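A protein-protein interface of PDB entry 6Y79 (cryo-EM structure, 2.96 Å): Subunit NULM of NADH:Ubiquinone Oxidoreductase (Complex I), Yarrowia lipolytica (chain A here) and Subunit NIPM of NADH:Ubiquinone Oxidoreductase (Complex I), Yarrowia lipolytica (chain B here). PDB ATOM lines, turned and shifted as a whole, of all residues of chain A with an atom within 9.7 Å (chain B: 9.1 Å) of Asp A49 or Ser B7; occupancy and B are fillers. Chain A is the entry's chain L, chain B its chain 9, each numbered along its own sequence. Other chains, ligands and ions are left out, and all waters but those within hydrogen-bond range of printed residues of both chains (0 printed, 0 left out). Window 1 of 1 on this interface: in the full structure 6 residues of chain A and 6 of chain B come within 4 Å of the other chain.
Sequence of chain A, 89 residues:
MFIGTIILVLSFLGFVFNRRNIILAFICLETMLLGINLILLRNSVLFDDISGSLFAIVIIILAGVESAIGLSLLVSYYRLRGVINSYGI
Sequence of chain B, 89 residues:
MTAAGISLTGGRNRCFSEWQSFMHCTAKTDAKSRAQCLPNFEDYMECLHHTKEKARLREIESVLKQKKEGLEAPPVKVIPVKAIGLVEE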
ATOM      1  N   LEU A  40      15.156  -5.608  24.950  1.00  0.00           N
ATOM      2  CA  LEU A  40      15.691  -6.437  23.877  1.00  0.00           C
ATOM      3  C   LEU A  40      15.829  -7.900  24.286  1.00  0.00           C
ATOM      4  O   LEU A  40      15.519  -8.803  23.497  1.00  0.00           O
ATOM      5  CB  LEU A  40      17.032  -5.882  23.448  1.00  0.00           C
ATOM      6  CG  LEU A  40      17.709  -6.688  22.375  1.00  0.00           C
ATOM      7  CD1 LEU A  40      16.889  -6.641  21.106  1.00  0.00           C
ATOM      8  CD2 LEU A  40      19.013  -6.057  22.212  1.00  0.00           C
ATOM      9  N   LEU A  41      16.292  -8.157  25.511  1.00  0.00           N
ATOM     10  CA  LEU A  41      16.494  -9.536  25.936  1.00  0.00           C
ATOM     11  C   LEU A  41      15.171 -10.246  26.165  1.00  0.00           C
ATOM     12  O   LEU A  41      15.057 -11.455  25.905  1.00  0.00           O
ATOM     13  CB  LEU A  41      17.368  -9.576  27.181  1.00  0.00           C
ATOM     14  CG  LEU A  41      18.840  -9.401  26.842  1.00  0.00           C
ATOM     15  CD1 LEU A  41      19.657  -9.422  28.091  1.00  0.00           C
ATOM     16  CD2 LEU A  41      19.289 -10.500  25.909  1.00  0.00           C
ATOM     17  N   ARG A  42      14.143  -9.506  26.598  1.00  0.00           N
ATOM     18  CA  ARG A  42      12.808 -10.089  26.629  1.00  0.00           C
ATOM     19  C   ARG A  42      12.329 -10.470  25.231  1.00  0.00           C
ATOM     20  O   ARG A  42      11.769 -11.552  25.043  1.00  0.00           O
ATOM     21  CB  ARG A  42      11.821  -9.129  27.282  1.00  0.00           C
ATOM     22  CG  ARG A  42      10.448  -9.736  27.456  1.00  0.00           C
ATOM     23  CD  ARG A  42       9.389  -8.690  27.362  1.00  0.00           C
ATOM     24  NE  ARG A  42       8.047  -9.253  27.385  1.00  0.00           N
ATOM     25  CZ  ARG A  42       7.350  -9.553  26.297  1.00  0.00           C
ATOM     26  NH1 ARG A  42       7.874  -9.336  25.101  1.00  0.00           N
ATOM     27  NH2 ARG A  42       6.131 -10.065  26.406  1.00  0.00           N
ATOM     28  N   ASN A  43      12.574  -9.616  24.231  1.00  0.00           N
ATOM     29  CA  ASN A  43      12.146  -9.941  22.866  1.00  0.00           C
ATOM     30  C   ASN A  43      12.902 -11.138  22.295  1.00  0.00           C
ATOM     31  O   ASN A  43      12.341 -11.927  21.525  1.00  0.00           O
ATOM     32  CB  ASN A  43      12.337  -8.722  21.969  1.00  0.00           C
ATOM     33  CG  ASN A  43      11.320  -7.658  22.238  1.00  0.00           C
ATOM     34  OD1 ASN A  43      10.136  -7.953  22.399  1.00  0.00           O
ATOM     35  ND2 ASN A  43      11.762  -6.414  22.319  1.00  0.00           N
ATOM     36  N   SER A  44      14.173 -11.280  22.662  1.00  0.00           N
ATOM     37  CA  SER A  44      14.963 -12.428  22.231  1.00  0.00           C
ATOM     38  C   SER A  44      14.435 -13.721  22.834  1.00  0.00           C
ATOM     39  O   SER A  44      14.405 -14.764  22.169  1.00  0.00           O
ATOM     40  CB  SER A  44      16.422 -12.222  22.621  1.00  0.00           C
ATOM     41  OG  SER A  44      17.209 -13.340  22.271  1.00  0.00           O
ATOM     42  N   VAL A  45      14.035 -13.674  24.108  1.00  0.00           N
ATOM     43  CA  VAL A  45      13.459 -14.850  24.756  1.00  0.00           C
ATOM     44  C   VAL A  45      12.111 -15.204  24.141  1.00  0.00           C
ATOM     45  O   VAL A  45      11.823 -16.376  23.873  1.00  0.00           O
ATOM     46  CB  VAL A  45      13.355 -14.603  26.271  1.00  0.00           C
ATOM     47  CG1 VAL A  45      12.418 -15.583  26.944  1.00  0.00           C
ATOM     48  CG2 VAL A  45      14.712 -14.706  26.881  1.00  0.00           C
ATOM     49  N   LEU A  46      11.281 -14.198  23.872  1.00  0.00           N
ATOM     50  CA  LEU A  46       9.965 -14.461  23.304  1.00  0.00           C
ATOM     51  C   LEU A  46      10.022 -14.934  21.855  1.00  0.00           C
ATOM     52  O   LEU A  46       9.148 -15.696  21.440  1.00  0.00           O
ATOM     53  CB  LEU A  46       9.071 -13.218  23.397  1.00  0.00           C
ATOM     54  CG  LEU A  46       8.153 -12.988  24.602  1.00  0.00           C
ATOM     55  CD1 LEU A  46       7.168 -14.124  24.746  1.00  0.00           C
ATOM     56  CD2 LEU A  46       8.902 -12.781  25.877  1.00  0.00           C
ATOM     57  N   PHE A  47      11.024 -14.524  21.076  1.00  0.00           N
ATOM     58  CA  PHE A  47      11.093 -14.918  19.672  1.00  0.00           C
ATOM     59  C   PHE A  47      11.907 -16.179  19.442  1.00  0.00           C
ATOM     60  O   PHE A  47      11.985 -16.629  18.294  1.00  0.00           O
ATOM     61  CB  PHE A  47      11.687 -13.796  18.814  1.00  0.00           C
ATOM     62  CG  PHE A  47      10.815 -12.583  18.702  1.00  0.00           C
ATOM     63  CD1 PHE A  47       9.458 -12.652  18.959  1.00  0.00           C
ATOM     64  CD2 PHE A  47      11.361 -11.366  18.353  1.00  0.00           C
ATOM     65  CE1 PHE A  47       8.671 -11.536  18.873  1.00  0.00           C
ATOM     66  CE2 PHE A  47      10.576 -10.250  18.263  1.00  0.00           C
ATOM     67  CZ  PHE A  47       9.232 -10.337  18.521  1.00  0.00           C
ATOM     68  N   ASP A  48      12.528 -16.724  20.501  1.00  0.00           N
ATOM     69  CA  ASP A  48      13.367 -17.934  20.482  1.00  0.00           C
ATOM     70  C   ASP A  48      14.606 -17.749  19.599  1.00  0.00           C
ATOM     71  O   ASP A  48      14.946 -18.612  18.800  1.00  0.00           O
ATOM     72  CB  ASP A  48      12.549 -19.172  20.057  1.00  0.00           C
ATOM     73  CG  ASP A  48      13.241 -20.504  20.359  1.00  0.00           C
ATOM     74  OD1 ASP A  48      14.303 -20.502  21.010  1.00  0.00           O
ATOM     75  OD2 ASP A  48      12.734 -21.549  19.903  1.00  0.00           O
ATOM     76  N   ASP A  49      15.318 -16.636  19.765  1.00  0.00           N
ATOM     77  CA  ASP A  49      16.529 -16.481  18.972  1.00  0.00           C
ATOM     78  C   ASP A  49      17.597 -15.682  19.703  1.00  0.00           C
ATOM     79  O   ASP A  49      17.336 -14.987  20.683  1.00  0.00           O
ATOM     80  CB  ASP A  49      16.244 -15.832  17.627  1.00  0.00           C
ATOM     81  CG  ASP A  49      15.644 -14.479  17.759  1.00  0.00           C
ATOM     82  OD1 ASP A  49      15.159 -14.112  18.844  1.00  0.00           O
ATOM     83  OD2 ASP A  49      15.690 -13.747  16.768  1.00  0.00           O
ATOM     84  N   ILE A  50      18.819 -15.796  19.178  1.00  0.00           N
ATOM     85  CA  ILE A  50      20.015 -15.208  19.771  1.00  0.00           C
ATOM     86  C   ILE A  50      20.350 -13.824  19.267  1.00  0.00           C
ATOM     87  O   ILE A  50      21.384 -13.274  19.667  1.00  0.00           O
ATOM     88  CB  ILE A  50      21.310 -15.945  19.412  1.00  0.00           C
ATOM     89  CG1 ILE A  50      21.272 -16.169  17.912  1.00  0.00           C
ATOM     90  CG2 ILE A  50      21.461 -17.208  20.191  1.00  0.00           C
ATOM     91  CD1 ILE A  50      22.573 -16.199  17.337  1.00  0.00           C
ATOM     92  N   SER A  51      19.580 -13.279  18.333  1.00  0.00           N
ATOM     93  CA  SER A  51      20.093 -12.143  17.584  1.00  0.00           C
ATOM     94  C   SER A  51      19.874 -10.867  18.367  1.00  0.00           C
ATOM     95  O   SER A  51      20.691  -9.936  18.312  1.00  0.00           O
ATOM     96  CB  SER A  51      19.429 -12.082  16.215  1.00  0.00           C
ATOM     97  OG  SER A  51      20.338 -11.553  15.310  1.00  0.00           O
ATOM     98  N   GLY A  52      18.766 -10.821  19.105  1.00  0.00           N
ATOM     99  CA  GLY A  52      18.634  -9.852  20.168  1.00  0.00           C
ATOM    100  C   GLY A  52      19.654 -10.048  21.271  1.00  0.00           C
ATOM    101  O   GLY A  52      20.162  -9.072  21.820  1.00  0.00           O
ATOM    102  N   SER A  53      20.021 -11.301  21.567  1.00  0.00           N
ATOM    103  CA  SER A  53      21.093 -11.544  22.528  1.00  0.00           C
ATOM    104  C   SER A  53      22.438 -11.089  21.970  1.00  0.00           C
ATOM    105  O   SER A  53      23.300 -10.641  22.728  1.00  0.00           O
ATOM    106  CB  SER A  53      21.138 -13.023  22.902  1.00  0.00           C
ATOM    107  OG  SER A  53      20.002 -13.406  23.654  1.00  0.00           O
ATOM    108  N   LEU A  54      22.614 -11.165  20.652  1.00  0.00           N
ATOM    109  CA  LEU A  54      23.826 -10.676  20.003  1.00  0.00           C
ATOM    110  C   LEU A  54      23.940  -9.161  20.115  1.00  0.00           C
ATOM    111  O   LEU A  54      24.989  -8.637  20.513  1.00  0.00           O
ATOM    112  CB  LEU A  54      23.811 -11.114  18.542  1.00  0.00           C
ATOM    113  CG  LEU A  54      24.989 -11.088  17.583  1.00  0.00           C
ATOM    114  CD1 LEU A  54      24.671 -12.155  16.616  1.00  0.00           C
ATOM    115  CD2 LEU A  54      25.072  -9.802  16.834  1.00  0.00           C
ATOM    116  N   PHE A  55      22.863  -8.440  19.772  1.00  0.00           N
ATOM    117  CA  PHE A  55      22.881  -6.985  19.907  1.00  0.00           C
ATOM    118  C   PHE A  55      23.005  -6.562  21.363  1.00  0.00           C
ATOM    119  O   PHE A  55      23.632  -5.541  21.654  1.00  0.00           O
ATOM    120  CB  PHE A  55      21.634  -6.374  19.264  1.00  0.00           C
ATOM    121  CG  PHE A  55      21.650  -4.861  19.181  1.00  0.00           C
ATOM    122  CD1 PHE A  55      22.307  -4.207  18.162  1.00  0.00           C
ATOM    123  CD2 PHE A  55      20.975  -4.097  20.113  1.00  0.00           C
ATOM    124  CE1 PHE A  55      22.304  -2.829  18.090  1.00  0.00           C
ATOM    125  CE2 PHE A  55      20.965  -2.722  20.047  1.00  0.00           C
ATOM    126  CZ  PHE A  55      21.630  -2.089  19.036  1.00  0.00           C
ATOM    127  N   ALA A  56      22.487  -7.369  22.293  1.00  0.00           N
ATOM    128  CA  ALA A  56      22.586  -7.039  23.711  1.00  0.00           C
ATOM    129  C   ALA A  56      24.003  -7.231  24.240  1.00  0.00           C
ATOM    130  O   ALA A  56      24.503  -6.398  25.006  1.00  0.00           O
ATOM    131  CB  ALA A  56      21.595  -7.874  24.512  1.00  0.00           C
ATOM    132  N   ALA B   3      22.793 -13.722  11.761  1.00  0.00           N
ATOM    133  CA  ALA B   3      21.992 -14.566  12.633  1.00  0.00           C
ATOM    134  C   ALA B   3      20.514 -14.402  12.301  1.00  0.00           C
ATOM    135  O   ALA B   3      19.719 -13.960  13.124  1.00  0.00           O
ATOM    136  CB  ALA B   3      22.252 -14.208  14.088  1.00  0.00           C
ATOM    137  N   ALA B   4      20.142 -14.792  11.085  1.00  0.00           N
ATOM    138  CA  ALA B   4      18.769 -14.566  10.645  1.00  0.00           C
ATOM    139  C   ALA B   4      17.807 -15.542  11.310  1.00  0.00           C
ATOM    140  O   ALA B   4      16.808 -15.132  11.911  1.00  0.00           O
ATOM    141  CB  ALA B   4      18.683 -14.664   9.125  1.00  0.00           C
ATOM    142  N   GLY B   5      18.096 -16.832  11.237  1.00  0.00           N
ATOM    143  CA  GLY B   5      17.190 -17.796  11.823  1.00  0.00           C
ATOM    144  C   GLY B   5      17.813 -18.676  12.879  1.00  0.00           C
ATOM    145  O   GLY B   5      17.366 -19.801  13.080  1.00  0.00           O
ATOM    146  N   ILE B   6      18.839 -18.188  13.559  1.00  0.00           N
ATOM    147  CA  ILE B   6      19.555 -18.974  14.553  1.00  0.00           C
ATOM    148  C   ILE B   6      18.868 -18.797  15.896  1.00  0.00           C
ATOM    149  O   ILE B   6      18.599 -17.670  16.316  1.00  0.00           O
ATOM    150  CB  ILE B   6      21.032 -18.556  14.619  1.00  0.00           C
ATOM    151  CG1 ILE B   6      21.639 -18.589  13.217  1.00  0.00           C
ATOM    152  CG2 ILE B   6      21.797 -19.459  15.552  1.00  0.00           C
ATOM    153  CD1 ILE B   6      23.065 -18.134  13.152  1.00  0.00           C
ATOM    154  N   SER B   7      18.575 -19.907  16.567  1.00  0.00           N
ATOM    155  CA  SER B   7      17.880 -19.878  17.843  1.00  0.00           C
ATOM    156  C   SER B   7      18.890 -19.887  18.986  1.00  0.00           C
ATOM    157  O   SER B   7      20.101 -19.866  18.764  1.00  0.00           O
ATOM    158  CB  SER B   7      16.917 -21.054  17.956  1.00  0.00           C
ATOM    159  OG  SER B   7      17.609 -22.274  18.097  1.00  0.00           O
ATOM    160  N   LEU B   8      18.382 -19.949  20.223  1.00  0.00           N
ATOM    161  CA  LEU B   8      19.224 -19.907  21.419  1.00  0.00           C
ATOM    162  C   LEU B   8      20.143 -21.113  21.512  1.00  0.00           C
ATOM    163  O   LEU B   8      21.260 -21.004  22.025  1.00  0.00           O
ATOM    164  CB  LEU B   8      18.355 -19.843  22.674  1.00  0.00           C
ATOM    165  CG  LEU B   8      17.821 -18.531  23.249  1.00  0.00           C
ATOM    166  CD1 LEU B   8      16.648 -18.081  22.462  1.00  0.00           C
ATOM    167  CD2 LEU B   8      17.388 -18.745  24.682  1.00  0.00           C
ATOM    168  N   THR B   9      19.700 -22.260  21.019  1.00  0.00           N
ATOM    169  CA  THR B   9      20.515 -23.459  20.998  1.00  0.00           C
ATOM    170  C   THR B   9      21.311 -23.588  19.717  1.00  0.00           C
ATOM    171  O   THR B   9      21.900 -24.640  19.480  1.00  0.00           O
ATOM    172  CB  THR B   9      19.642 -24.696  21.166  1.00  0.00           C
ATOM    173  OG1 THR B   9      19.059 -25.038  19.900  1.00  0.00           O
ATOM    174  CG2 THR B   9      18.534 -24.427  22.171  1.00  0.00           C
ATOM    175  N   GLY B  10      21.321 -22.564  18.877  1.00  0.00           N
ATOM    176  CA  GLY B  10      21.960 -22.678  17.593  1.00  0.00           C
ATOM    177  C   GLY B  10      21.134 -23.326  16.522  1.00  0.00           C
ATOM    178  O   GLY B  10      21.594 -23.404  15.380  1.00  0.00           O
ATOM    179  N   GLY B  11      19.945 -23.807  16.846  1.00  0.00           N
ATOM    180  CA  GLY B  11      19.048 -24.368  15.864  1.00  0.00           C
ATOM    181  C   GLY B  11      18.262 -23.287  15.158  1.00  0.00           C
ATOM    182  O   GLY B  11      18.643 -22.116  15.135  1.00  0.00           O
ATOM    183  N   ARG B  12      17.145 -23.686  14.572  1.00  0.00           N
ATOM    184  CA  ARG B  12      16.258 -22.732  13.929  1.00  0.00           C
ATOM    185  C   ARG B  12      15.276 -22.175  14.953  1.00  0.00           C
ATOM    186  O   ARG B  12      14.923 -22.847  15.923  1.00  0.00           O
ATOM    187  CB  ARG B  12      15.535 -23.390  12.756  1.00  0.00           C
ATOM    188  CG  ARG B  12      16.489 -23.872  11.676  1.00  0.00           C
ATOM    189  CD  ARG B  12      15.887 -24.913  10.792  1.00  0.00           C
ATOM    190  NE  ARG B  12      16.687 -25.162   9.604  1.00  0.00           N
ATOM    191  CZ  ARG B  12      16.205 -25.615   8.453  1.00  0.00           C
ATOM    192  NH1 ARG B  12      14.921 -25.870   8.338  1.00  0.00           N
ATOM    193  NH2 ARG B  12      17.012 -25.812   7.417  1.00  0.00           N
ATOM    194  N   ASN B  13      14.854 -20.926  14.756  1.00  0.00           N
ATOM    195  CA  ASN B  13      14.037 -20.279  15.775  1.00  0.00           C
ATOM    196  C   ASN B  13      12.590 -20.757  15.665  1.00  0.00           C
ATOM    197  O   ASN B  13      12.260 -21.670  14.906  1.00  0.00           O
ATOM    198  CB  ASN B  13      14.187 -18.753  15.732  1.00  0.00           C
ATOM    199  CG  ASN B  13      13.913 -18.138  14.389  1.00  0.00           C
ATOM    200  OD1 ASN B  13      13.371 -18.754  13.501  1.00  0.00           O
ATOM    201  ND2 ASN B  13      14.278 -16.877  14.251  1.00  0.00           N
ATOM    202  N   ARG B  14      11.709 -20.148  16.455  1.00  0.00           N
ATOM    203  CA  ARG B  14      10.341 -20.634  16.552  1.00  0.00           C
ATOM    204  C   ARG B  14       9.545 -20.344  15.288  1.00  0.00           C
ATOM    205  O   ARG B  14       8.703 -21.153  14.887  1.00  0.00           O
ATOM    206  CB  ARG B  14       9.669 -20.007  17.762  1.00  0.00           C
ATOM    207  CG  ARG B  14       8.372 -20.636  18.148  1.00  0.00           C
ATOM    208  CD  ARG B  14       7.767 -19.849  19.267  1.00  0.00           C
ATOM    209  NE  ARG B  14       7.568 -18.464  18.873  1.00  0.00           N
ATOM    210  CZ  ARG B  14       7.270 -17.494  19.722  1.00  0.00           C
ATOM    211  NH1 ARG B  14       7.105 -16.258  19.285  1.00  0.00           N
ATOM    212  NH2 ARG B  14       7.142 -17.762  21.014  1.00  0.00           N
ATOM    213  N   CYS B  15       9.806 -19.218  14.635  1.00  0.00           N
ATOM    214  CA  CYS B  15       9.094 -18.834  13.427  1.00  0.00           C
ATOM    215  C   CYS B  15       9.955 -18.971  12.186  1.00  0.00           C
ATOM    216  O   CYS B  15       9.808 -18.197  11.241  1.00  0.00           O
ATOM    217  CB  CYS B  15       8.583 -17.407  13.535  1.00  0.00           C
ATOM    218  SG  CYS B  15       7.342 -17.206  14.775  1.00  0.00           S
ATOM    219  N   PHE B  16      10.873 -19.933  12.185  1.00  0.00           N
ATOM    220  CA  PHE B  16      11.722 -20.117  11.021  1.00  0.00           C
ATOM    221  C   PHE B  16      10.945 -20.658   9.843  1.00  0.00           C
ATOM    222  O   PHE B  16      11.240 -20.307   8.696  1.00  0.00           O
ATOM    223  CB  PHE B  16      12.875 -21.057  11.331  1.00  0.00           C
ATOM    224  CG  PHE B  16      13.821 -21.210  10.203  1.00  0.00           C
ATOM    225  CD1 PHE B  16      14.684 -20.187   9.879  1.00  0.00           C
ATOM    226  CD2 PHE B  16      13.830 -22.357   9.446  1.00  0.00           C
ATOM    227  CE1 PHE B  16      15.551 -20.315   8.838  1.00  0.00           C
ATOM    228  CE2 PHE B  16      14.704 -22.486   8.413  1.00  0.00           C
ATOM    229  CZ  PHE B  16      15.555 -21.463   8.105  1.00  0.00           C
ATOM    230  N   TRP B  19       8.748 -18.064   8.154  1.00  0.00           N
ATOM    231  CA  TRP B  19       9.614 -17.126   7.456  1.00  0.00           C
ATOM    232  C   TRP B  19      10.202 -17.739   6.198  1.00  0.00           C
ATOM    233  O   TRP B  19      10.311 -17.061   5.177  1.00  0.00           O
ATOM    234  CB  TRP B  19      10.738 -16.646   8.362  1.00  0.00           C
ATOM    235  CG  TRP B  19      11.535 -15.567   7.713  1.00  0.00           C
ATOM    236  CD1 TRP B  19      11.051 -14.538   6.971  1.00  0.00           C
ATOM    237  CD2 TRP B  19      12.954 -15.418   7.727  1.00  0.00           C
ATOM    238  NE1 TRP B  19      12.074 -13.752   6.522  1.00  0.00           N
ATOM    239  CE2 TRP B  19      13.257 -14.271   6.973  1.00  0.00           C
ATOM    240  CE3 TRP B  19      13.999 -16.141   8.304  1.00  0.00           C
ATOM    241  CZ2 TRP B  19      14.559 -13.830   6.779  1.00  0.00           C
ATOM    242  CZ3 TRP B  19      15.288 -15.695   8.121  1.00  0.00           C
ATOM    243  CH2 TRP B  19      15.559 -14.555   7.357  1.00  0.00           C
ATOM    244  N   TYR B  44       3.365 -15.350   9.092  1.00  0.00           N
ATOM    245  CA  TYR B  44       4.592 -15.073   9.810  1.00  0.00           C
ATOM    246  C   TYR B  44       4.329 -14.148  10.981  1.00  0.00           C
ATOM    247  O   TYR B  44       4.808 -14.403  12.092  1.00  0.00           O
ATOM    248  CB  TYR B  44       5.625 -14.468   8.877  1.00  0.00           C
ATOM    249  CG  TYR B  44       6.917 -14.213   9.578  1.00  0.00           C
ATOM    250  CD1 TYR B  44       7.605 -15.252  10.175  1.00  0.00           C
ATOM    251  CD2 TYR B  44       7.445 -12.937   9.666  1.00  0.00           C
ATOM    252  CE1 TYR B  44       8.782 -15.033  10.832  1.00  0.00           C
ATOM    253  CE2 TYR B  44       8.626 -12.710  10.320  1.00  0.00           C
ATOM    254  CZ  TYR B  44       9.290 -13.765  10.897  1.00  0.00           C
ATOM    255  OH  TYR B  44      10.473 -13.563  11.549  1.00  0.00           O
ATOM    256  N   LEU B  48       4.752 -14.555  15.107  1.00  0.00           N
ATOM    257  CA  LEU B  48       5.588 -13.784  16.012  1.00  0.00           C
ATOM    258  C   LEU B  48       4.812 -13.364  17.248  1.00  0.00           C
ATOM    259  O   LEU B  48       5.255 -13.577  18.380  1.00  0.00           O
ATOM    260  CB  LEU B  48       6.130 -12.555  15.288  1.00  0.00           C
ATOM    261  CG  LEU B  48       7.150 -12.753  14.182  1.00  0.00           C
ATOM    262  CD1 LEU B  48       7.434 -11.417  13.546  1.00  0.00           C
ATOM    263  CD2 LEU B  48       8.407 -13.360  14.745  1.00  0.00           C
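The side-chain amide oxygen (OD1) of Asn B13 is in hydrogen-bond range of the backbone NH (N) of Phe B16.
O of Ser A44 is in hydrogen-bond range of N of Asp A49 (3.2 Å).
O of Leu B48 sits at hydrogen-bond distance from NH1 of Arg B14.
The side-chain hydroxyl (OG) of Ser B7 sits at hydrogen-bond distance from the backbone NH (N) of Gly B11 (3.1 Å).
The backbone NH of Asn B13 sits at hydrogen-bond distance from the backbone carbonyl oxygen of Gly B5, 3.2 Å away.
Of the printed residues of chain B, Phe A47 touches Asn B13 (3.99 Å) and Arg B14 (3.98 Å).
Asp A48 touches four residues of chain B.
Ile A50 touches four residues of chain B.
Ser B7 touches just these residues of chain A: Asp A48 (3.2 Å), Asp A49 (3.8 Å) and Ile A50 (3.3 Å).
Of the printed residues of chain A, Leu B8 touches Asp A48 (3.5 Å), Asp A49 (3.3 Å) and Ile A50 (3.7 Å).
Thr B9 touches none of the printed residues of chain A.
Of the printed residues of chain A, Asn B13 touches Phe A47 and Asp A48.
The nearest printed residue of chain A that does not touch Ser B7 is Ser A51 (6.6 Å).
Of the 17 printed residues of chain B, 6 touch a printed residue of chain A.
Hydrophobic or aromatic side chains of chain A that line the printed part of chain B: Ile A50.
Among the printed residues, no Asp or Glu carboxylate lies within 4 Å of a Lys or Arg side-chain nitrogen of the other chain.
O of Phe A47 touches CB of Asn B13, 3.99 Å away.
O of Phe A47 touches N of Arg B14 (3.98 Å).
O of Asp A48 touches CB of Ser B7 (3.2 Å).
C of Asp A48 touches CD1 of Leu B8, at 3.5 Å.
Asp A48 touches Asn B13 (O to CB, 3.2 Å).
Arg B14 touches Asp A48 (CB to CB, 3.8 Å).
CB of Asp A49 touches O of Ile B6 (3.3 Å).
Asp A49 touches Ser B7.
CD1 of Leu B8 touches N of Asp A49, 3.3 Å away.
CA of Leu B8 touches CG2 of Ile A50, at 3.7 Å.
O of Leu A46 sits at hydrogen-bond distance from NH2 of Arg B14.
The side-chain hydroxyl (OG) of Ser A51 sits at hydrogen-bond distance from the backbone carbonyl oxygen (O) of Ala B3, at 3.3 Å.
The backbone NH (N) of Ile A50 lies within hydrogen-bond range of the backbone carbonyl oxygen (O) of Ile B6, at 3.4 Å.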
